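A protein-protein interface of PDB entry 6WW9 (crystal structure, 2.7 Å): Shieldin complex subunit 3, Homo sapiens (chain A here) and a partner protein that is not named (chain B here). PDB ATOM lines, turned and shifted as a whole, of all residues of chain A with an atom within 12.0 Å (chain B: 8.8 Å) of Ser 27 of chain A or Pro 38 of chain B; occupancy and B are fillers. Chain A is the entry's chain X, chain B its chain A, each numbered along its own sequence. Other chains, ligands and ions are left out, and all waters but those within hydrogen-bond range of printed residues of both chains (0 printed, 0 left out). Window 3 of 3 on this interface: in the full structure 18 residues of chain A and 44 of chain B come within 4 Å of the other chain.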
ATOM      1  N   SER A  23      12.476 -38.580 -23.769  1.00  0.00           N
ATOM      2  CA  SER A  23      11.557 -37.727 -24.499  1.00  0.00           C
ATOM      3  C   SER A  23      11.943 -36.264 -24.319  1.00  0.00           C
ATOM      4  O   SER A  23      12.465 -35.881 -23.266  1.00  0.00           O
ATOM      5  CB  SER A  23      10.113 -37.940 -24.027  1.00  0.00           C
ATOM      6  OG  SER A  23       9.709 -39.283 -24.234  1.00  0.00           O
ATOM      7  N   PRO A  24      11.715 -35.428 -25.328  1.00  0.00           N
ATOM      8  CA  PRO A  24      12.046 -34.007 -25.203  1.00  0.00           C
ATOM      9  C   PRO A  24      11.146 -33.333 -24.185  1.00  0.00           C
ATOM     10  O   PRO A  24      10.079 -33.865 -23.842  1.00  0.00           O
ATOM     11  CB  PRO A  24      11.799 -33.463 -26.619  1.00  0.00           C
ATOM     12  CG  PRO A  24      10.796 -34.392 -27.196  1.00  0.00           C
ATOM     13  CD  PRO A  24      11.144 -35.745 -26.648  1.00  0.00           C
ATOM     14  N   PRO A  25      11.543 -32.170 -23.672  1.00  0.00           N
ATOM     15  CA  PRO A  25      10.710 -31.487 -22.676  1.00  0.00           C
ATOM     16  C   PRO A  25       9.379 -31.055 -23.273  1.00  0.00           C
ATOM     17  O   PRO A  25       9.301 -30.639 -24.430  1.00  0.00           O
ATOM     18  CB  PRO A  25      11.560 -30.278 -22.269  1.00  0.00           C
ATOM     19  CG  PRO A  25      12.955 -30.632 -22.680  1.00  0.00           C
ATOM     20  CD  PRO A  25      12.805 -31.454 -23.916  1.00  0.00           C
ATOM     21  N   ALA A  26       8.325 -31.170 -22.471  1.00  0.00           N
ATOM     22  CA  ALA A  26       7.004 -30.752 -22.916  1.00  0.00           C
ATOM     23  C   ALA A  26       6.938 -29.233 -23.040  1.00  0.00           C
ATOM     24  O   ALA A  26       7.603 -28.496 -22.307  1.00  0.00           O
ATOM     25  CB  ALA A  26       5.930 -31.246 -21.947  1.00  0.00           C
ATOM     26  N   SER A  27       6.129 -28.767 -23.984  1.00  0.00           N
ATOM     27  CA  SER A  27       6.002 -27.335 -24.227  1.00  0.00           C
ATOM     28  C   SER A  27       5.207 -26.654 -23.116  1.00  0.00           C
ATOM     29  O   SER A  27       4.404 -27.291 -22.434  1.00  0.00           O
ATOM     30  CB  SER A  27       5.343 -27.077 -25.585  1.00  0.00           C
ATOM     31  OG  SER A  27       4.108 -27.761 -25.694  1.00  0.00           O
ATOM     32  N   LEU B  31      10.531 -27.526 -35.513  1.00  0.00           N
ATOM     33  CA  LEU B  31       9.780 -27.274 -34.288  1.00  0.00           C
ATOM     34  C   LEU B  31       9.170 -25.879 -34.282  1.00  0.00           C
ATOM     35  O   LEU B  31       8.109 -25.666 -33.684  1.00  0.00           O
ATOM     36  CB  LEU B  31      10.683 -27.459 -33.068  1.00  0.00           C
ATOM     37  CG  LEU B  31      11.300 -28.844 -32.876  1.00  0.00           C
ATOM     38  CD1 LEU B  31      12.095 -28.891 -31.582  1.00  0.00           C
ATOM     39  CD2 LEU B  31      10.224 -29.916 -32.888  1.00  0.00           C
ATOM     40  N   TYR B  32       9.821 -24.920 -34.944  1.00  0.00           N
ATOM     41  CA  TYR B  32       9.275 -23.572 -35.039  1.00  0.00           C
ATOM     42  C   TYR B  32       8.162 -23.490 -36.079  1.00  0.00           C
ATOM     43  O   TYR B  32       7.093 -22.931 -35.810  1.00  0.00           O
ATOM     44  CB  TYR B  32      10.388 -22.575 -35.373  1.00  0.00           C
ATOM     45  CG  TYR B  32       9.911 -21.143 -35.462  1.00  0.00           C
ATOM     46  CD1 TYR B  32       9.683 -20.398 -34.313  1.00  0.00           C
ATOM     47  CD2 TYR B  32       9.690 -20.535 -36.691  1.00  0.00           C
ATOM     48  CE1 TYR B  32       9.246 -19.090 -34.383  1.00  0.00           C
ATOM     49  CE2 TYR B  32       9.251 -19.221 -36.772  1.00  0.00           C
ATOM     50  CZ  TYR B  32       9.032 -18.504 -35.613  1.00  0.00           C
ATOM     51  OH  TYR B  32       8.597 -17.199 -35.676  1.00  0.00           O
ATOM     52  N   ARG B  34       6.315 -25.892 -37.507  1.00  0.00           N
ATOM     53  CA  ARG B  34       5.168 -26.706 -37.135  1.00  0.00           C
ATOM     54  C   ARG B  34       4.645 -26.374 -35.746  1.00  0.00           C
ATOM     55  O   ARG B  34       3.687 -27.011 -35.293  1.00  0.00           O
ATOM     56  CB  ARG B  34       5.521 -28.194 -37.227  1.00  0.00           C
ATOM     57  CG  ARG B  34       5.921 -28.634 -38.628  1.00  0.00           C
ATOM     58  CD  ARG B  34       5.000 -28.030 -39.685  1.00  0.00           C
ATOM     59  NE  ARG B  34       3.667 -28.628 -39.681  1.00  0.00           N
ATOM     60  CZ  ARG B  34       2.578 -28.022 -40.143  1.00  0.00           C
ATOM     61  NH1 ARG B  34       2.661 -26.793 -40.633  1.00  0.00           N
ATOM     62  NH2 ARG B  34       1.404 -28.638 -40.106  1.00  0.00           N
ATOM     63  N   GLU B  35       5.254 -25.399 -35.068  1.00  0.00           N
ATOM     64  CA  GLU B  35       4.723 -24.844 -33.823  1.00  0.00           C
ATOM     65  C   GLU B  35       4.664 -25.890 -32.714  1.00  0.00           C
ATOM     66  O   GLU B  35       3.716 -25.932 -31.928  1.00  0.00           O
ATOM     67  CB  GLU B  35       3.347 -24.215 -34.047  1.00  0.00           C
ATOM     68  CG  GLU B  35       3.360 -23.052 -35.019  1.00  0.00           C
ATOM     69  CD  GLU B  35       2.009 -22.380 -35.137  1.00  0.00           C
ATOM     70  OE1 GLU B  35       0.982 -23.091 -35.139  1.00  0.00           O
ATOM     71  OE2 GLU B  35       1.972 -21.137 -35.223  1.00  0.00           O
ATOM     72  N   VAL B  36       5.692 -26.738 -32.636  1.00  0.00           N
ATOM     73  CA  VAL B  36       5.746 -27.716 -31.558  1.00  0.00           C
ATOM     74  C   VAL B  36       6.068 -27.046 -30.229  1.00  0.00           C
ATOM     75  O   VAL B  36       5.747 -27.591 -29.166  1.00  0.00           O
ATOM     76  CB  VAL B  36       6.764 -28.823 -31.895  1.00  0.00           C
ATOM     77  CG1 VAL B  36       6.641 -29.983 -30.925  1.00  0.00           C
ATOM     78  CG2 VAL B  36       6.557 -29.308 -33.318  1.00  0.00           C
ATOM     79  N   TYR B  37       6.668 -25.863 -30.261  1.00  0.00           N
ATOM     80  CA  TYR B  37       7.039 -25.133 -29.061  1.00  0.00           C
ATOM     81  C   TYR B  37       6.683 -23.663 -29.233  1.00  0.00           C
ATOM     82  O   TYR B  37       6.631 -23.163 -30.363  1.00  0.00           O
ATOM     83  CB  TYR B  37       8.538 -25.284 -28.761  1.00  0.00           C
ATOM     84  CG  TYR B  37       8.907 -26.649 -28.227  1.00  0.00           C
ATOM     85  CD1 TYR B  37       8.670 -26.980 -26.900  1.00  0.00           C
ATOM     86  CD2 TYR B  37       9.493 -27.606 -29.046  1.00  0.00           C
ATOM     87  CE1 TYR B  37       9.003 -28.225 -26.402  1.00  0.00           C
ATOM     88  CE2 TYR B  37       9.832 -28.855 -28.557  1.00  0.00           C
ATOM     89  CZ  TYR B  37       9.585 -29.159 -27.234  1.00  0.00           C
ATOM     90  OH  TYR B  37       9.920 -30.401 -26.741  1.00  0.00           O
ATOM     91  N   PRO B  38       6.429 -22.950 -28.134  1.00  0.00           N
ATOM     92  CA  PRO B  38       6.037 -21.540 -28.244  1.00  0.00           C
ATOM     93  C   PRO B  38       7.159 -20.678 -28.802  1.00  0.00           C
ATOM     94  O   PRO B  38       8.343 -21.001 -28.684  1.00  0.00           O
ATOM     95  CB  PRO B  38       5.711 -21.145 -26.797  1.00  0.00           C
ATOM     96  CG  PRO B  38       5.530 -22.439 -26.061  1.00  0.00           C
ATOM     97  CD  PRO B  38       6.436 -23.413 -26.737  1.00  0.00           C
ATOM     98  N   VAL B  39       6.761 -19.554 -29.407  1.00  0.00           N
ATOM     99  CA  VAL B  39       7.718 -18.648 -30.033  1.00  0.00           C
ATOM    100  C   VAL B  39       8.691 -18.067 -29.016  1.00  0.00           C
ATOM    101  O   VAL B  39       9.796 -17.650 -29.383  1.00  0.00           O
ATOM    102  CB  VAL B  39       6.976 -17.517 -30.783  1.00  0.00           C
ATOM    103  CG1 VAL B  39       5.931 -18.095 -31.710  1.00  0.00           C
ATOM    104  CG2 VAL B  39       6.346 -16.546 -29.802  1.00  0.00           C
ATOM    105  N   GLY B  40       8.309 -18.032 -27.738  1.00  0.00           N
ATOM    106  CA  GLY B  40       9.132 -17.390 -26.728  1.00  0.00           C
ATOM    107  C   GLY B  40      10.472 -18.056 -26.501  1.00  0.00           C
ATOM    108  O   GLY B  40      11.400 -17.407 -26.004  1.00  0.00           O
ATOM    109  N   ILE B  41      10.604 -19.339 -26.857  1.00  0.00           N
ATOM    110  CA  ILE B  41      11.865 -20.046 -26.662  1.00  0.00           C
ATOM    111  C   ILE B  41      12.742 -20.030 -27.905  1.00  0.00           C
ATOM    112  O   ILE B  41      13.844 -20.594 -27.880  1.00  0.00           O
ATOM    113  CB  ILE B  41      11.630 -21.507 -26.231  1.00  0.00           C
ATOM    114  CG1 ILE B  41      11.085 -22.328 -27.400  1.00  0.00           C
ATOM    115  CG2 ILE B  41      10.679 -21.563 -25.048  1.00  0.00           C
ATOM    116  CD1 ILE B  41      11.490 -23.784 -27.358  1.00  0.00           C
ATOM    117  N   PHE B  42      12.293 -19.400 -28.988  1.00  0.00           N
ATOM    118  CA  PHE B  42      13.046 -19.327 -30.229  1.00  0.00           C
ATOM    119  C   PHE B  42      13.644 -17.940 -30.410  1.00  0.00           C
ATOM    120  O   PHE B  42      13.053 -16.930 -30.015  1.00  0.00           O
ATOM    121  CB  PHE B  42      12.166 -19.661 -31.437  1.00  0.00           C
ATOM    122  CG  PHE B  42      11.725 -21.094 -31.488  1.00  0.00           C
ATOM    123  CD1 PHE B  42      12.557 -22.070 -32.008  1.00  0.00           C
ATOM    124  CD2 PHE B  42      10.475 -21.462 -31.023  1.00  0.00           C
ATOM    125  CE1 PHE B  42      12.154 -23.389 -32.056  1.00  0.00           C
ATOM    126  CE2 PHE B  42      10.066 -22.780 -31.067  1.00  0.00           C
ATOM    127  CZ  PHE B  42      10.906 -23.745 -31.586  1.00  0.00           C
ATOM    128  N   GLN B  43      14.827 -17.905 -31.017  1.00  0.00           N
ATOM    129  CA  GLN B  43      15.496 -16.665 -31.373  1.00  0.00           C
ATOM    130  C   GLN B  43      16.022 -16.770 -32.795  1.00  0.00           C
ATOM    131  O   GLN B  43      16.341 -17.860 -33.279  1.00  0.00           O
ATOM    132  CB  GLN B  43      16.647 -16.342 -30.418  1.00  0.00           C
ATOM    133  CG  GLN B  43      16.204 -15.801 -29.077  1.00  0.00           C
ATOM    134  CD  GLN B  43      17.372 -15.328 -28.243  1.00  0.00           C
ATOM    135  OE1 GLN B  43      18.494 -15.213 -28.736  1.00  0.00           O
ATOM    136  NE2 GLN B  43      17.118 -15.054 -26.969  1.00  0.00           N
ATOM    137  N   GLN B  53      15.326 -19.879 -37.065  1.00  0.00           N
ATOM    138  CA  GLN B  53      14.806 -19.737 -35.710  1.00  0.00           C
ATOM    139  C   GLN B  53      15.371 -20.877 -34.873  1.00  0.00           C
ATOM    140  O   GLN B  53      14.989 -22.037 -35.054  1.00  0.00           O
ATOM    141  CB  GLN B  53      13.279 -19.736 -35.707  1.00  0.00           C
ATOM    142  CG  GLN B  53      12.657 -18.483 -36.311  1.00  0.00           C
ATOM    143  CD  GLN B  53      12.670 -17.298 -35.359  1.00  0.00           C
ATOM    144  OE1 GLN B  53      13.329 -17.327 -34.320  1.00  0.00           O
ATOM    145  NE2 GLN B  53      11.933 -16.252 -35.710  1.00  0.00           N
ATOM    146  N   MET B  54      16.288 -20.544 -33.970  1.00  0.00           N
ATOM    147  CA  MET B  54      16.950 -21.526 -33.127  1.00  0.00           C
ATOM    148  C   MET B  54      16.329 -21.525 -31.737  1.00  0.00           C
ATOM    149  O   MET B  54      15.961 -20.472 -31.207  1.00  0.00           O
ATOM    150  CB  MET B  54      18.450 -21.239 -33.029  1.00  0.00           C
ATOM    151  CG  MET B  54      19.179 -21.285 -34.364  1.00  0.00           C
ATOM    152  SD  MET B  54      19.209 -22.927 -35.113  1.00  0.00           S
ATOM    153  CE  MET B  54      20.300 -23.800 -33.989  1.00  0.00           C
ATOM    154  N   SER B  55      16.209 -22.713 -31.156  1.00  0.00           N
ATOM    155  CA  SER B  55      15.691 -22.830 -29.803  1.00  0.00           C
ATOM    156  C   SER B  55      16.740 -22.389 -28.792  1.00  0.00           C
ATOM    157  O   SER B  55      17.921 -22.729 -28.906  1.00  0.00           O
ATOM    158  CB  SER B  55      15.266 -24.268 -29.517  1.00  0.00           C
ATOM    159  OG  SER B  55      15.100 -24.474 -28.126  1.00  0.00           O
ATOM    160  N   CYS B  56      16.299 -21.618 -27.799  1.00  0.00           N
ATOM    161  CA  CYS B  56      17.133 -21.236 -26.668  1.00  0.00           C
ATOM    162  C   CYS B  56      16.743 -21.975 -25.396  1.00  0.00           C
ATOM    163  O   CYS B  56      17.189 -21.601 -24.306  1.00  0.00           O
ATOM    164  CB  CYS B  56      17.073 -19.724 -26.449  1.00  0.00           C
ATOM    165  SG  CYS B  56      17.840 -18.771 -27.778  1.00  0.00           S
ATOM    166  N   HIS B  57      15.924 -23.010 -25.514  1.00  0.00           N
ATOM    167  CA  HIS B  57      15.573 -23.841 -24.373  1.00  0.00           C
ATOM    168  C   HIS B  57      16.717 -24.805 -24.081  1.00  0.00           C
ATOM    169  O   HIS B  57      17.063 -25.618 -24.945  1.00  0.00           O
ATOM    170  CB  HIS B  57      14.289 -24.607 -24.662  1.00  0.00           C
ATOM    171  CG  HIS B  57      13.629 -25.168 -23.444  1.00  0.00           C
ATOM    172  ND1 HIS B  57      14.106 -26.279 -22.786  1.00  0.00           N
ATOM    173  CD2 HIS B  57      12.522 -24.777 -22.770  1.00  0.00           C
ATOM    174  CE1 HIS B  57      13.325 -26.547 -21.755  1.00  0.00           C
ATOM    175  NE2 HIS B  57      12.356 -25.651 -21.723  1.00  0.00           N
ATOM    176  N   LEU B  60      15.738 -28.629 -24.138  1.00  0.00           N
ATOM    177  CA  LEU B  60      15.394 -29.015 -25.501  1.00  0.00           C
ATOM    178  C   LEU B  60      16.636 -29.088 -26.379  1.00  0.00           C
ATOM    179  O   LEU B  60      16.783 -30.018 -27.181  1.00  0.00           O
ATOM    180  CB  LEU B  60      14.379 -28.032 -26.087  1.00  0.00           C
ATOM    181  CG  LEU B  60      13.996 -28.264 -27.551  1.00  0.00           C
ATOM    182  CD1 LEU B  60      13.358 -29.631 -27.727  1.00  0.00           C
ATOM    183  CD2 LEU B  60      13.062 -27.171 -28.039  1.00  0.00           C
ATOM    184  N   LYS B  90      -1.287 -35.727 -29.053  1.00  0.00           N
ATOM    185  CA  LYS B  90      -1.355 -35.974 -27.616  1.00  0.00           C
ATOM    186  C   LYS B  90      -1.657 -37.427 -27.278  1.00  0.00           C
ATOM    187  O   LYS B  90      -1.528 -37.811 -26.110  1.00  0.00           O
ATOM    188  CB  LYS B  90      -2.400 -35.056 -26.980  1.00  0.00           C
ATOM    189  CG  LYS B  90      -1.804 -34.021 -26.039  1.00  0.00           C
ATOM    190  CD  LYS B  90      -2.780 -32.890 -25.752  1.00  0.00           C
ATOM    191  CE  LYS B  90      -2.135 -31.814 -24.891  1.00  0.00           C
ATOM    192  NZ  LYS B  90      -2.976 -30.588 -24.798  1.00  0.00           N
ATOM    193  N   PRO B 142      -3.238 -29.347 -31.252  1.00  0.00           N
ATOM    194  CA  PRO B 142      -2.497 -28.762 -30.130  1.00  0.00           C
ATOM    195  C   PRO B 142      -1.915 -29.833 -29.220  1.00  0.00           C
ATOM    196  O   PRO B 142      -2.445 -30.940 -29.099  1.00  0.00           O
ATOM    197  CB  PRO B 142      -3.557 -27.930 -29.402  1.00  0.00           C
ATOM    198  CG  PRO B 142      -4.843 -28.620 -29.725  1.00  0.00           C
ATOM    199  CD  PRO B 142      -4.691 -29.135 -31.129  1.00  0.00           C
ATOM    200  N   GLY B 143      -0.801 -29.487 -28.579  1.00  0.00           N
ATOM    201  CA  GLY B 143      -0.169 -30.383 -27.629  1.00  0.00           C
ATOM    202  C   GLY B 143       0.684 -31.474 -28.231  1.00  0.00           C
ATOM    203  O   GLY B 143       0.881 -32.512 -27.591  1.00  0.00           O
ATOM    204  N   CYS B 144       1.207 -31.275 -29.436  1.00  0.00           N
ATOM    205  CA  CYS B 144       2.025 -32.290 -30.083  1.00  0.00           C
ATOM    206  C   CYS B 144       3.430 -32.322 -29.489  1.00  0.00           C
ATOM    207  O   CYS B 144       3.943 -31.316 -28.990  1.00  0.00           O
ATOM    208  CB  CYS B 144       2.107 -32.041 -31.591  1.00  0.00           C
ATOM    209  SG  CYS B 144       0.628 -32.519 -32.518  1.00  0.00           S
ATOM    210  N   THR B 145       4.046 -33.498 -29.548  1.00  0.00           N
ATOM    211  CA  THR B 145       5.440 -33.710 -29.174  1.00  0.00           C
ATOM    212  C   THR B 145       6.205 -34.209 -30.396  1.00  0.00           C
ATOM    213  O   THR B 145       5.659 -34.298 -31.499  1.00  0.00           O
ATOM    214  CB  THR B 145       5.561 -34.697 -28.007  1.00  0.00           C
ATOM    215  OG1 THR B 145       4.966 -35.950 -28.365  1.00  0.00           O
ATOM    216  CG2 THR B 145       4.869 -34.151 -26.766  1.00  0.00           C
ATOM    217  N   PHE B 146       7.480 -34.540 -30.203  1.00  0.00           N
ATOM    218  CA  PHE B 146       8.278 -35.011 -31.323  1.00  0.00           C
ATOM    219  C   PHE B 146       9.313 -36.022 -30.851  1.00  0.00           C
ATOM    220  O   PHE B 146       9.676 -36.075 -29.673  1.00  0.00           O
ATOM    221  CB  PHE B 146       8.969 -33.855 -32.059  1.00  0.00           C
ATOM    222  CG  PHE B 146      10.302 -33.464 -31.479  1.00  0.00           C
ATOM    223  CD1 PHE B 146      10.377 -32.586 -30.411  1.00  0.00           C
ATOM    224  CD2 PHE B 146      11.483 -33.952 -32.023  1.00  0.00           C
ATOM    225  CE1 PHE B 146      11.598 -32.215 -29.887  1.00  0.00           C
ATOM    226  CE2 PHE B 146      12.708 -33.584 -31.499  1.00  0.00           C
ATOM    227  CZ  PHE B 146      12.764 -32.715 -30.430  1.00  0.00           C
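Of the 24 printed residues of chain B, 5 touch a printed residue of chain A.
Printed residues of chain B that touch a printed residue of chain A: Val 36, Tyr 37, Pro 38, Leu 60 and Phe 146.
Hydrophobic or aromatic side chains of chain B that line the printed part of chain A: Tyr 37, Pro 38 and Phe 146.
Of the 5 printed residues of chain A, 3 touch a printed residue of chain B.
Hydrophobic or aromatic side chains of chain A that line the printed part of chain B: Pro 24 and Pro 25.
Among the printed residues, no Asp or Glu carboxylate lies within 4 Å of a Lys or Arg side-chain nitrogen of the other chain.
Of the printed residues of chain B, Ser 27 of chain A touches Val 36, Tyr 37 and Pro 38.
Printed residues of chain A within 4 Å of Pro 38 of chain B: Ser 27.
No residue of chain B comes within 4 Å of Ala 26 of chain A.
No residue of chain A comes within 4 Å of Gly 40 of chain B.
No residue of chain A comes within 4 Å of Gly 143 of chain B.
Of the printed residues of chain B, Pro 24 of chain A touches Tyr 37 (3.6 Å) and Phe 146 (3.2 Å).
Of the printed residues of chain B, Pro 25 of chain A touches Tyr 37 and Leu 60.
Printed residues of chain A within 4 Å of Phe 146 of chain B: Pro 24.
Of the printed residues of chain A, Val 36 of chain B touches Ser 27.
Met 54 of chain B touches none of the printed residues of chain A.
Glu 35 of chain B touches none of the printed residues of chain A.
The nearest printed residue of chain B that does not touch Ser 27 of chain A is Cys 144 of chain B (4.9 Å).
The nearest printed residue of chain A that does not touch Pro 38 of chain B is Ala 26 of chain A (6.8 Å).
Among the printed residues, pairs that only touch across the chains: Pro 24 of chain A with Tyr 37 of chain B (3.6 Å), Pro 24 of chain A with Phe 146 of chain B (3.2 Å), Pro 25 of chain A with Leu 60 of chain B (3.7 Å), Ser 27 of chain A with Val 36 of chain B (3.6 Å), Ser 27 of chain A with Tyr 37 of chain B (3.6 Å) and Ser 27 of chain A with Pro 38 of chain B (3.99 Å).
The backbone carbonyl oxygen (O) of Pro 25 of chain A is in hydrogen-bond range of the side-chain hydroxyl (OH) of Tyr 37 of chain B, at 2.4 Å.
A ring nitrogen (ND1) of His 57 of chain B lies within hydrogen-bond range of the backbone NH (N) of Leu 60 of chain B (3.2 Å).
The backbone carbonyl oxygen of Leu 31 of chain B lies within hydrogen-bond range of the backbone NH of Val 36 of chain B.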
